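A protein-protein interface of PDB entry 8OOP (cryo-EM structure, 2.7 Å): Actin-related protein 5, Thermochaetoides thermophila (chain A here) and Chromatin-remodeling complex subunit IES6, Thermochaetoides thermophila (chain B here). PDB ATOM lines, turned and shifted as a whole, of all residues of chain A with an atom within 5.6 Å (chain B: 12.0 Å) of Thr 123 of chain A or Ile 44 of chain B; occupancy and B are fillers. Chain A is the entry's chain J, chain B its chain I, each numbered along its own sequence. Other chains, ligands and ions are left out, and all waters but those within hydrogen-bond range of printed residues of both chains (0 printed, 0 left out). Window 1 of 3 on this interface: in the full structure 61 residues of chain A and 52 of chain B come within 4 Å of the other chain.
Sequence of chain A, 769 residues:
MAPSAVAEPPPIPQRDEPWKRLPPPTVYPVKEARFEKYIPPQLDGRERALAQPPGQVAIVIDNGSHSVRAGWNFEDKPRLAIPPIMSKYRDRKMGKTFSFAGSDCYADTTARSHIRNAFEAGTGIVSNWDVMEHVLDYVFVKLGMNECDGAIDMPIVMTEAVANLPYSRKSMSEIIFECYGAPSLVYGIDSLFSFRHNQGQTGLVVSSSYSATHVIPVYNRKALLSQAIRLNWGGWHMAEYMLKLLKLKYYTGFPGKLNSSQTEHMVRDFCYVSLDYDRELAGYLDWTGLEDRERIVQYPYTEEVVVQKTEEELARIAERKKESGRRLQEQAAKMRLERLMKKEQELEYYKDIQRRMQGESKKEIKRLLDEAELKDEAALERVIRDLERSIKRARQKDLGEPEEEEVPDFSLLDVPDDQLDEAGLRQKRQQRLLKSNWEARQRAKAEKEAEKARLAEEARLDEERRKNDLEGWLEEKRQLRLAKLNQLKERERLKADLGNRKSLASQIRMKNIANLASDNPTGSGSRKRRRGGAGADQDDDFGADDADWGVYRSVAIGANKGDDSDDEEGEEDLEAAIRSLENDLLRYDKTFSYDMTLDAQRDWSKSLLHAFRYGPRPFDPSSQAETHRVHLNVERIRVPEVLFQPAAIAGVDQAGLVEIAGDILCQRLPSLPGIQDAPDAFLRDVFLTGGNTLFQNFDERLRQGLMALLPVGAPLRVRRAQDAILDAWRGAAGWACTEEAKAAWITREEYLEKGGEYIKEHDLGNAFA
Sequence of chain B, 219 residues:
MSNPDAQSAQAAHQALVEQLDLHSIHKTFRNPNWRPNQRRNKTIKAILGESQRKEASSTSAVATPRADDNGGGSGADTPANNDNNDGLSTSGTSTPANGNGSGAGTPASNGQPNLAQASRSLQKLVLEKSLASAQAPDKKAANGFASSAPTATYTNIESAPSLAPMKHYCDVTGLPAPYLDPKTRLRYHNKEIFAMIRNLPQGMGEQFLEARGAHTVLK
OD1 of Asn 41 of chain B lies close to O of Ser 127 of chain A (3.5 Å).
The backbone NH of Ile 44 of chain B lies within hydrogen-bond range of the side-chain carboxylate of Glu 120 of chain A (2.9 Å).
NZ of Lys 42 of chain B lies within salt-bridge range of OE2 of Glu 50 of chain B (2.7 Å).
The backbone NH (N) of Ala 46 of chain B lies within hydrogen-bond range of the side-chain hydroxyl (OG1) of Thr 43 of chain B, 3.1 Å away.
The side-chain hydroxyl (OG) of Ser 51 of chain B sits at hydrogen-bond distance from the backbone carbonyl oxygen (O) of Leu 48 of chain B (2.7 Å).
The backbone carbonyl oxygen (O) of Leu 48 of chain B sits close to the side-chain amide oxygen (OE1) of Gln 52 of chain B, 3.2 Å away.
The backbone carbonyl oxygen of Glu 120 of chain A is in hydrogen-bond range of the side-chain hydroxyl of Thr 123 of chain A (2.8 Å).
The side-chain hydroxyl (OG) of Ser 127 of chain A lies within hydrogen-bond range of the backbone NH (N) of Glu 120 of chain A, 3.4 Å away.
Glu 120 of chain A touches Thr 43 of chain B.
CD1 of Ile 44 of chain B touches OG1 of Thr 123 of chain A (3.3 Å).
Ile 125 of chain A touches Ile 44 of chain B.
O of Lys 42 of chain B touches CB of Ser 127 of chain A, at 3.6 Å.
Ile 47 of chain B touches Leu 165 of chain A (CG2 to CD1, 3.7 Å).
Leu 48 of chain B touches Leu 165 of chain A (CD1 to CD2, 3.9 Å).
OD1 of Asn 156 of chain B touches CD2 of Leu 165 of chain A (3.9 Å).
Ser 65 of chain A touches none of the printed residues of chain B.
Ala 121 of chain A touches none of the printed residues of chain B.
No residue of chain B comes within 4 Å of Gly 122 of chain A.
Thr 123 of chain A touches just one residue of chain B: Ile 44.
Ile 125 of chain A touches one residue of chain B.
Ser 127 of chain A touches two residues of chain B.
Of the printed residues of chain B, Leu 165 of chain A touches Ile 47, Leu 48 and Asn 156.
Ser 211 of chain A touches none of the printed residues of chain B.
Arg 40 of chain B touches none of the printed residues of chain A.
Ile 44 of chain B touches three residues of chain A.
Of the printed residues of chain A, Ile 47 of chain B touches Leu 165.
The nearest residue of chain B that does not touch Thr 123 of chain A is Asn 156 of chain B (7.3 Å).
The nearest residue of chain A that does not touch Ile 44 of chain B is Leu 165 of chain A (4.3 Å).
Of the 19 printed residues of chain B, 7 touch a printed residue of chain A.
Hydrophobic or aromatic side chains of chain B within 4 Å of the printed part of chain A: Ile 44, Ile 47 and Leu 48.
Of the 12 printed residues of chain A, 5 touch a printed residue of chain B.
Among the printed residues, no Asp or Glu carboxylate lies within 4 Å of a Lys or Arg side-chain nitrogen of the other chain.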
ATOM      1  N   SER A  65      16.002 -40.376  11.220  1.00  0.00           N
ATOM      2  CA  SER A  65      16.586 -40.221  12.553  1.00  0.00           C
ATOM      3  C   SER A  65      16.093 -41.264  13.552  1.00  0.00           C
ATOM      4  O   SER A  65      16.800 -41.572  14.518  1.00  0.00           O
ATOM      5  CB  SER A  65      16.280 -38.825  13.099  1.00  0.00           C
ATOM      6  OG  SER A  65      16.632 -37.813  12.176  1.00  0.00           O
ATOM      7  N   PHE A 119      22.789 -38.519  14.367  1.00  0.00           N
ATOM      8  CA  PHE A 119      22.113 -37.228  14.292  1.00  0.00           C
ATOM      9  C   PHE A 119      22.384 -36.383  15.531  1.00  0.00           C
ATOM     10  O   PHE A 119      22.568 -36.904  16.634  1.00  0.00           O
ATOM     11  CB  PHE A 119      20.608 -37.420  14.098  1.00  0.00           C
ATOM     12  CG  PHE A 119      20.249 -38.055  12.784  1.00  0.00           C
ATOM     13  CD1 PHE A 119      20.287 -39.429  12.630  1.00  0.00           C
ATOM     14  CD2 PHE A 119      19.871 -37.277  11.702  1.00  0.00           C
ATOM     15  CE1 PHE A 119      19.967 -40.016  11.424  1.00  0.00           C
ATOM     16  CE2 PHE A 119      19.539 -37.861  10.493  1.00  0.00           C
ATOM     17  CZ  PHE A 119      19.591 -39.233  10.353  1.00  0.00           C
ATOM     18  N   GLU A 120      22.408 -35.066  15.337  1.00  0.00           N
ATOM     19  CA  GLU A 120      22.382 -34.156  16.475  1.00  0.00           C
ATOM     20  C   GLU A 120      21.039 -34.263  17.182  1.00  0.00           C
ATOM     21  O   GLU A 120      19.983 -34.173  16.548  1.00  0.00           O
ATOM     22  CB  GLU A 120      22.644 -32.718  16.035  1.00  0.00           C
ATOM     23  CG  GLU A 120      22.476 -31.715  17.166  1.00  0.00           C
ATOM     24  CD  GLU A 120      23.280 -30.446  16.966  1.00  0.00           C
ATOM     25  OE1 GLU A 120      24.320 -30.498  16.278  1.00  0.00           O
ATOM     26  OE2 GLU A 120      22.883 -29.397  17.516  1.00  0.00           O
ATOM     27  N   ALA A 121      21.090 -34.467  18.497  1.00  0.00           N
ATOM     28  CA  ALA A 121      19.925 -34.888  19.268  1.00  0.00           C
ATOM     29  C   ALA A 121      18.747 -33.934  19.106  1.00  0.00           C
ATOM     30  O   ALA A 121      18.863 -32.728  19.339  1.00  0.00           O
ATOM     31  CB  ALA A 121      20.304 -35.003  20.743  1.00  0.00           C
ATOM     32  N   GLY A 122      17.606 -34.493  18.707  1.00  0.00           N
ATOM     33  CA  GLY A 122      16.404 -33.722  18.468  1.00  0.00           C
ATOM     34  C   GLY A 122      16.381 -32.917  17.196  1.00  0.00           C
ATOM     35  O   GLY A 122      15.592 -31.974  17.093  1.00  0.00           O
ATOM     36  N   THR A 123      17.222 -33.252  16.223  1.00  0.00           N
ATOM     37  CA  THR A 123      17.247 -32.565  14.940  1.00  0.00           C
ATOM     38  C   THR A 123      17.361 -33.602  13.833  1.00  0.00           C
ATOM     39  O   THR A 123      17.760 -34.746  14.065  1.00  0.00           O
ATOM     40  CB  THR A 123      18.399 -31.547  14.836  1.00  0.00           C
ATOM     41  OG1 THR A 123      19.636 -32.234  14.621  1.00  0.00           O
ATOM     42  CG2 THR A 123      18.506 -30.680  16.091  1.00  0.00           C
ATOM     43  N   GLY A 124      17.000 -33.190  12.624  1.00  0.00           N
ATOM     44  CA  GLY A 124      17.014 -34.055  11.466  1.00  0.00           C
ATOM     45  C   GLY A 124      18.340 -34.119  10.741  1.00  0.00           C
ATOM     46  O   GLY A 124      18.417 -34.749   9.680  1.00  0.00           O
ATOM     47  N   ILE A 125      19.389 -33.504  11.281  1.00  0.00           N
ATOM     48  CA  ILE A 125      20.645 -33.300  10.569  1.00  0.00           C
ATOM     49  C   ILE A 125      21.676 -34.299  11.079  1.00  0.00           C
ATOM     50  O   ILE A 125      21.876 -34.434  12.292  1.00  0.00           O
ATOM     51  CB  ILE A 125      21.150 -31.857  10.742  1.00  0.00           C
ATOM     52  CG1 ILE A 125      20.039 -30.869  10.396  1.00  0.00           C
ATOM     53  CG2 ILE A 125      22.364 -31.602   9.863  1.00  0.00           C
ATOM     54  CD1 ILE A 125      19.503 -31.006   8.991  1.00  0.00           C
ATOM     55  N   SER A 127      25.328 -35.395  11.961  1.00  0.00           N
ATOM     56  CA  SER A 127      26.497 -34.667  12.446  1.00  0.00           C
ATOM     57  C   SER A 127      27.614 -35.553  12.978  1.00  0.00           C
ATOM     58  O   SER A 127      28.754 -35.081  13.047  1.00  0.00           O
ATOM     59  CB  SER A 127      26.094 -33.671  13.541  1.00  0.00           C
ATOM     60  OG  SER A 127      25.641 -34.343  14.702  1.00  0.00           O
ATOM     61  N   LEU A 165      21.485 -28.757   5.681  1.00  0.00           N
ATOM     62  CA  LEU A 165      22.661 -27.894   5.671  1.00  0.00           C
ATOM     63  C   LEU A 165      23.652 -28.324   4.588  1.00  0.00           C
ATOM     64  O   LEU A 165      23.912 -29.519   4.425  1.00  0.00           O
ATOM     65  CB  LEU A 165      23.345 -27.909   7.033  1.00  0.00           C
ATOM     66  CG  LEU A 165      22.468 -27.523   8.220  1.00  0.00           C
ATOM     67  CD1 LEU A 165      23.268 -27.580   9.503  1.00  0.00           C
ATOM     68  CD2 LEU A 165      21.917 -26.122   7.996  1.00  0.00           C
ATOM     69  N   SER A 211      12.208 -36.252  14.330  1.00  0.00           N
ATOM     70  CA  SER A 211      12.991 -35.045  14.581  1.00  0.00           C
ATOM     71  C   SER A 211      12.190 -33.745  14.596  1.00  0.00           C
ATOM     72  O   SER A 211      12.596 -32.795  15.276  1.00  0.00           O
ATOM     73  CB  SER A 211      14.098 -34.910  13.533  1.00  0.00           C
ATOM     74  OG  SER A 211      13.562 -34.623  12.253  1.00  0.00           O
ATOM     75  N   HIS A 237      11.144 -35.396  20.794  1.00  0.00           N
ATOM     76  CA  HIS A 237      10.796 -34.405  21.808  1.00  0.00           C
ATOM     77  C   HIS A 237       9.678 -34.886  22.723  1.00  0.00           C
ATOM     78  O   HIS A 237       9.687 -34.610  23.929  1.00  0.00           O
ATOM     79  CB  HIS A 237      10.380 -33.111  21.118  1.00  0.00           C
ATOM     80  CG  HIS A 237      11.427 -32.548  20.210  1.00  0.00           C
ATOM     81  ND1 HIS A 237      12.262 -31.518  20.574  1.00  0.00           N
ATOM     82  CD2 HIS A 237      11.783 -32.889  18.952  1.00  0.00           C
ATOM     83  CE1 HIS A 237      13.080 -31.242  19.574  1.00  0.00           C
ATOM     84  NE2 HIS A 237      12.809 -32.061  18.578  1.00  0.00           N
ATOM     85  N   ARG B  39      38.047 -34.283  12.522  1.00  0.00           N
ATOM     86  CA  ARG B  39      37.181 -33.305  13.176  1.00  0.00           C
ATOM     87  C   ARG B  39      36.033 -32.809  12.295  1.00  0.00           C
ATOM     88  O   ARG B  39      35.529 -31.702  12.506  1.00  0.00           O
ATOM     89  CB  ARG B  39      38.012 -32.151  13.737  1.00  0.00           C
ATOM     90  CG  ARG B  39      38.977 -32.657  14.804  1.00  0.00           C
ATOM     91  CD  ARG B  39      39.516 -31.558  15.700  1.00  0.00           C
ATOM     92  NE  ARG B  39      40.403 -32.109  16.720  1.00  0.00           N
ATOM     93  CZ  ARG B  39      41.701 -32.329  16.567  1.00  0.00           C
ATOM     94  NH1 ARG B  39      42.327 -32.031  15.441  1.00  0.00           N
ATOM     95  NH2 ARG B  39      42.391 -32.863  17.573  1.00  0.00           N
ATOM     96  N   ARG B  40      35.624 -33.604  11.307  1.00  0.00           N
ATOM     97  CA  ARG B  40      34.446 -33.311  10.495  1.00  0.00           C
ATOM     98  C   ARG B  40      33.134 -33.258  11.286  1.00  0.00           C
ATOM     99  O   ARG B  40      32.162 -32.679  10.791  1.00  0.00           O
ATOM    100  CB  ARG B  40      34.366 -34.353   9.379  1.00  0.00           C
ATOM    101  CG  ARG B  40      34.173 -35.769   9.899  1.00  0.00           C
ATOM    102  CD  ARG B  40      34.123 -36.803   8.787  1.00  0.00           C
ATOM    103  NE  ARG B  40      34.183 -38.152   9.334  1.00  0.00           N
ATOM    104  CZ  ARG B  40      33.936 -39.259   8.647  1.00  0.00           C
ATOM    105  NH1 ARG B  40      33.597 -39.221   7.370  1.00  0.00           N
ATOM    106  NH2 ARG B  40      34.038 -40.437   9.257  1.00  0.00           N
ATOM    107  N   ASN B  41      33.073 -33.839  12.487  1.00  0.00           N
ATOM    108  CA  ASN B  41      31.826 -33.925  13.253  1.00  0.00           C
ATOM    109  C   ASN B  41      31.369 -32.616  13.903  1.00  0.00           C
ATOM    110  O   ASN B  41      31.094 -32.582  15.108  1.00  0.00           O
ATOM    111  CB  ASN B  41      31.951 -35.004  14.330  1.00  0.00           C
ATOM    112  CG  ASN B  41      32.181 -36.378  13.748  1.00  0.00           C
ATOM    113  OD1 ASN B  41      31.809 -36.652  12.608  1.00  0.00           O
ATOM    114  ND2 ASN B  41      32.788 -37.260  14.530  1.00  0.00           N
ATOM    115  N   LYS B  42      31.279 -31.546  13.119  1.00  0.00           N
ATOM    116  CA  LYS B  42      30.782 -30.262  13.609  1.00  0.00           C
ATOM    117  C   LYS B  42      29.306 -30.318  13.999  1.00  0.00           C
ATOM    118  O   LYS B  42      28.504 -31.013  13.369  1.00  0.00           O
ATOM    119  CB  LYS B  42      30.989 -29.196  12.539  1.00  0.00           C
ATOM    120  CG  LYS B  42      32.443 -28.984  12.195  1.00  0.00           C
ATOM    121  CD  LYS B  42      32.655 -27.718  11.400  1.00  0.00           C
ATOM    122  CE  LYS B  42      34.119 -27.578  11.027  1.00  0.00           C
ATOM    123  NZ  LYS B  42      34.439 -26.217  10.529  1.00  0.00           N
ATOM    124  N   THR B  43      28.955 -29.587  15.060  1.00  0.00           N
ATOM    125  CA  THR B  43      27.563 -29.397  15.452  1.00  0.00           C
ATOM    126  C   THR B  43      26.848 -28.420  14.518  1.00  0.00           C
ATOM    127  O   THR B  43      27.471 -27.658  13.775  1.00  0.00           O
ATOM    128  CB  THR B  43      27.471 -28.875  16.887  1.00  0.00           C
ATOM    129  OG1 THR B  43      28.108 -27.593  16.970  1.00  0.00           O
ATOM    130  CG2 THR B  43      28.153 -29.833  17.853  1.00  0.00           C
ATOM    131  N   ILE B  44      25.511 -28.448  14.578  1.00  0.00           N
ATOM    132  CA  ILE B  44      24.688 -27.489  13.840  1.00  0.00           C
ATOM    133  C   ILE B  44      25.059 -26.054  14.195  1.00  0.00           C
ATOM    134  O   ILE B  44      25.146 -25.184  13.319  1.00  0.00           O
ATOM    135  CB  ILE B  44      23.194 -27.759  14.105  1.00  0.00           C
ATOM    136  CG1 ILE B  44      22.763 -29.085  13.476  1.00  0.00           C
ATOM    137  CG2 ILE B  44      22.332 -26.611  13.592  1.00  0.00           C
ATOM    138  CD1 ILE B  44      21.403 -29.555  13.935  1.00  0.00           C
ATOM    139  N   LYS B  45      25.269 -25.780  15.484  1.00  0.00           N
ATOM    140  CA  LYS B  45      25.760 -24.476  15.918  1.00  0.00           C
ATOM    141  C   LYS B  45      27.053 -24.096  15.205  1.00  0.00           C
ATOM    142  O   LYS B  45      27.193 -22.980  14.692  1.00  0.00           O
ATOM    143  CB  LYS B  45      25.949 -24.484  17.436  1.00  0.00           C
ATOM    144  CG  LYS B  45      26.751 -23.328  18.010  1.00  0.00           C
ATOM    145  CD  LYS B  45      26.807 -23.443  19.527  1.00  0.00           C
ATOM    146  CE  LYS B  45      28.049 -22.791  20.110  1.00  0.00           C
ATOM    147  NZ  LYS B  45      28.045 -21.313  19.947  1.00  0.00           N
ATOM    148  N   ALA B  46      28.012 -25.021  15.165  1.00  0.00           N
ATOM    149  CA  ALA B  46      29.282 -24.771  14.491  1.00  0.00           C
ATOM    150  C   ALA B  46      29.115 -24.630  12.981  1.00  0.00           C
ATOM    151  O   ALA B  46      29.759 -23.777  12.359  1.00  0.00           O
ATOM    152  CB  ALA B  46      30.271 -25.888  14.814  1.00  0.00           C
ATOM    153  N   ILE B  47      28.254 -25.450  12.375  1.00  0.00           N
ATOM    154  CA  ILE B  47      28.022 -25.372  10.933  1.00  0.00           C
ATOM    155  C   ILE B  47      27.383 -24.041  10.549  1.00  0.00           C
ATOM    156  O   ILE B  47      27.794 -23.397   9.577  1.00  0.00           O
ATOM    157  CB  ILE B  47      27.163 -26.560  10.468  1.00  0.00           C
ATOM    158  CG1 ILE B  47      27.929 -27.870  10.649  1.00  0.00           C
ATOM    159  CG2 ILE B  47      26.762 -26.390   9.010  1.00  0.00           C
ATOM    160  CD1 ILE B  47      27.046 -29.093  10.651  1.00  0.00           C
ATOM    161  N   LEU B  48      26.371 -23.608  11.302  1.00  0.00           N
ATOM    162  CA  LEU B  48      25.810 -22.274  11.092  1.00  0.00           C
ATOM    163  C   LEU B  48      26.845 -21.177  11.311  1.00  0.00           C
ATOM    164  O   LEU B  48      26.758 -20.112  10.690  1.00  0.00           O
ATOM    165  CB  LEU B  48      24.604 -22.062  12.005  1.00  0.00           C
ATOM    166  CG  LEU B  48      23.226 -22.417  11.438  1.00  0.00           C
ATOM    167  CD1 LEU B  48      23.184 -23.837  10.890  1.00  0.00           C
ATOM    168  CD2 LEU B  48      22.163 -22.219  12.504  1.00  0.00           C
ATOM    169  N   GLY B  49      27.824 -21.413  12.183  1.00  0.00           N
ATOM    170  CA  GLY B  49      28.962 -20.518  12.329  1.00  0.00           C
ATOM    171  C   GLY B  49      29.842 -20.384  11.098  1.00  0.00           C
ATOM    172  O   GLY B  49      30.702 -19.495  11.075  1.00  0.00           O
ATOM    173  N   GLU B  50      29.653 -21.224  10.082  1.00  0.00           N
ATOM    174  CA  GLU B  50      30.315 -21.023   8.798  1.00  0.00           C
ATOM    175  C   GLU B  50      29.557 -20.089   7.863  1.00  0.00           C
ATOM    176  O   GLU B  50      30.093 -19.733   6.808  1.00  0.00           O
ATOM    177  CB  GLU B  50      30.541 -22.369   8.100  1.00  0.00           C
ATOM    178  CG  GLU B  50      31.297 -23.375   8.948  1.00  0.00           C
ATOM    179  CD  GLU B  50      31.904 -24.491   8.124  1.00  0.00           C
ATOM    180  OE1 GLU B  50      31.420 -24.735   7.000  1.00  0.00           O
ATOM    181  OE2 GLU B  50      32.868 -25.125   8.605  1.00  0.00           O
ATOM    182  N   SER B  51      28.334 -19.688   8.215  1.00  0.00           N
ATOM    183  CA  SER B  51      27.582 -18.782   7.356  1.00  0.00           C
ATOM    184  C   SER B  51      28.203 -17.391   7.317  1.00  0.00           C
ATOM    185  O   SER B  51      28.077 -16.686   6.310  1.00  0.00           O
ATOM    186  CB  SER B  51      26.134 -18.687   7.832  1.00  0.00           C
ATOM    187  OG  SER B  51      26.062 -18.055   9.099  1.00  0.00           O
ATOM    188  N   GLN B  52      28.867 -16.982   8.392  1.00  0.00           N
ATOM    189  CA  GLN B  52      29.543 -15.691   8.436  1.00  0.00           C
ATOM    190  C   GLN B  52      30.800 -15.686   7.570  1.00  0.00           C
ATOM    191  O   GLN B  52      31.729 -16.459   7.801  1.00  0.00           O
ATOM    192  CB  GLN B  52      29.890 -15.323   9.881  1.00  0.00           C
ATOM    193  CG  GLN B  52      28.674 -15.069  10.762  1.00  0.00           C
ATOM    194  CD  GLN B  52      28.060 -16.346  11.303  1.00  0.00           C
ATOM    195  OE1 GLN B  52      28.518 -17.447  10.999  1.00  0.00           O
ATOM    196  NE2 GLN B  52      27.011 -16.204  12.107  1.00  0.00           N
ATOM    197  N   THR B 155      16.165 -22.527   4.408  1.00  0.00           N
ATOM    198  CA  THR B 155      17.587 -22.621   4.713  1.00  0.00           C
ATOM    199  C   THR B 155      17.842 -22.583   6.217  1.00  0.00           C
ATOM    200  O   THR B 155      18.701 -21.838   6.691  1.00  0.00           O
ATOM    201  CB  THR B 155      18.385 -21.497   4.031  1.00  0.00           C
ATOM    202  OG1 THR B 155      18.030 -20.234   4.605  1.00  0.00           O
ATOM    203  CG2 THR B 155      18.101 -21.468   2.534  1.00  0.00           C
ATOM    204  N   ASN B 156      17.074 -23.390   6.957  1.00  0.00           N
ATOM    205  CA  ASN B 156      16.944 -23.274   8.415  1.00  0.00           C
ATOM    206  C   ASN B 156      16.525 -21.870   8.850  1.00  0.00           C
ATOM    207  O   ASN B 156      16.951 -21.368   9.891  1.00  0.00           O
ATOM    208  CB  ASN B 156      18.224 -23.722   9.123  1.00  0.00           C
ATOM    209  CG  ASN B 156      18.328 -25.232   9.217  1.00  0.00           C
ATOM    210  OD1 ASN B 156      18.045 -25.944   8.256  1.00  0.00           O
ATOM    211  ND2 ASN B 156      18.694 -25.731  10.391  1.00  0.00           N
ATOM    212  N   ILE B 157      15.703 -21.226   8.025  1.00  0.00           N
ATOM    213  CA  ILE B 157      14.988 -19.996   8.357  1.00  0.00           C
ATOM    214  C   ILE B 157      13.491 -20.282   8.305  1.00  0.00           C
ATOM    215  O   ILE B 157      12.680 -19.388   8.043  1.00  0.00           O
ATOM    216  CB  ILE B 157      15.387 -18.834   7.429  1.00  0.00           C
ATOM    217  CG1 ILE B 157      14.995 -19.135   5.978  1.00  0.00           C
ATOM    218  CG2 ILE B 157      16.873 -18.518   7.565  1.00  0.00           C
ATOM    219  CD1 ILE B 157      15.216 -17.970   5.037  1.00  0.00           C
ATOM    220  N   GLU B 158      13.128 -21.541   8.527  1.00  0.00           N
ATOM    221  CA  GLU B 158      11.760 -22.031   8.420  1.00  0.00           C
ATOM    222  C   GLU B 158      10.985 -22.009   9.739  1.00  0.00           C
ATOM    223  O   GLU B 158       9.809 -22.387   9.752  1.00  0.00           O
ATOM    224  CB  GLU B 158      11.802 -23.459   7.884  1.00  0.00           C
ATOM    225  CG  GLU B 158      12.490 -23.572   6.551  1.00  0.00           C
ATOM    226  CD  GLU B 158      12.263 -24.913   5.910  1.00  0.00           C
ATOM    227  OE1 GLU B 158      12.120 -25.900   6.656  1.00  0.00           O
ATOM    228  OE2 GLU B 158      12.223 -24.982   4.664  1.00  0.00           O
ATOM    229  N   SER B 159      11.617 -21.622  10.842  1.00  0.00           N
ATOM    230  CA  SER B 159      10.967 -21.546  12.147  1.00  0.00           C
ATOM    231  C   SER B 159      10.007 -20.355  12.253  1.00  0.00           C
ATOM    232  O   SER B 159      10.223 -19.305  11.643  1.00  0.00           O
ATOM    233  CB  SER B 159      12.035 -21.475  13.236  1.00  0.00           C
ATOM    234  OG  SER B 159      12.991 -22.511  13.060  1.00  0.00           O
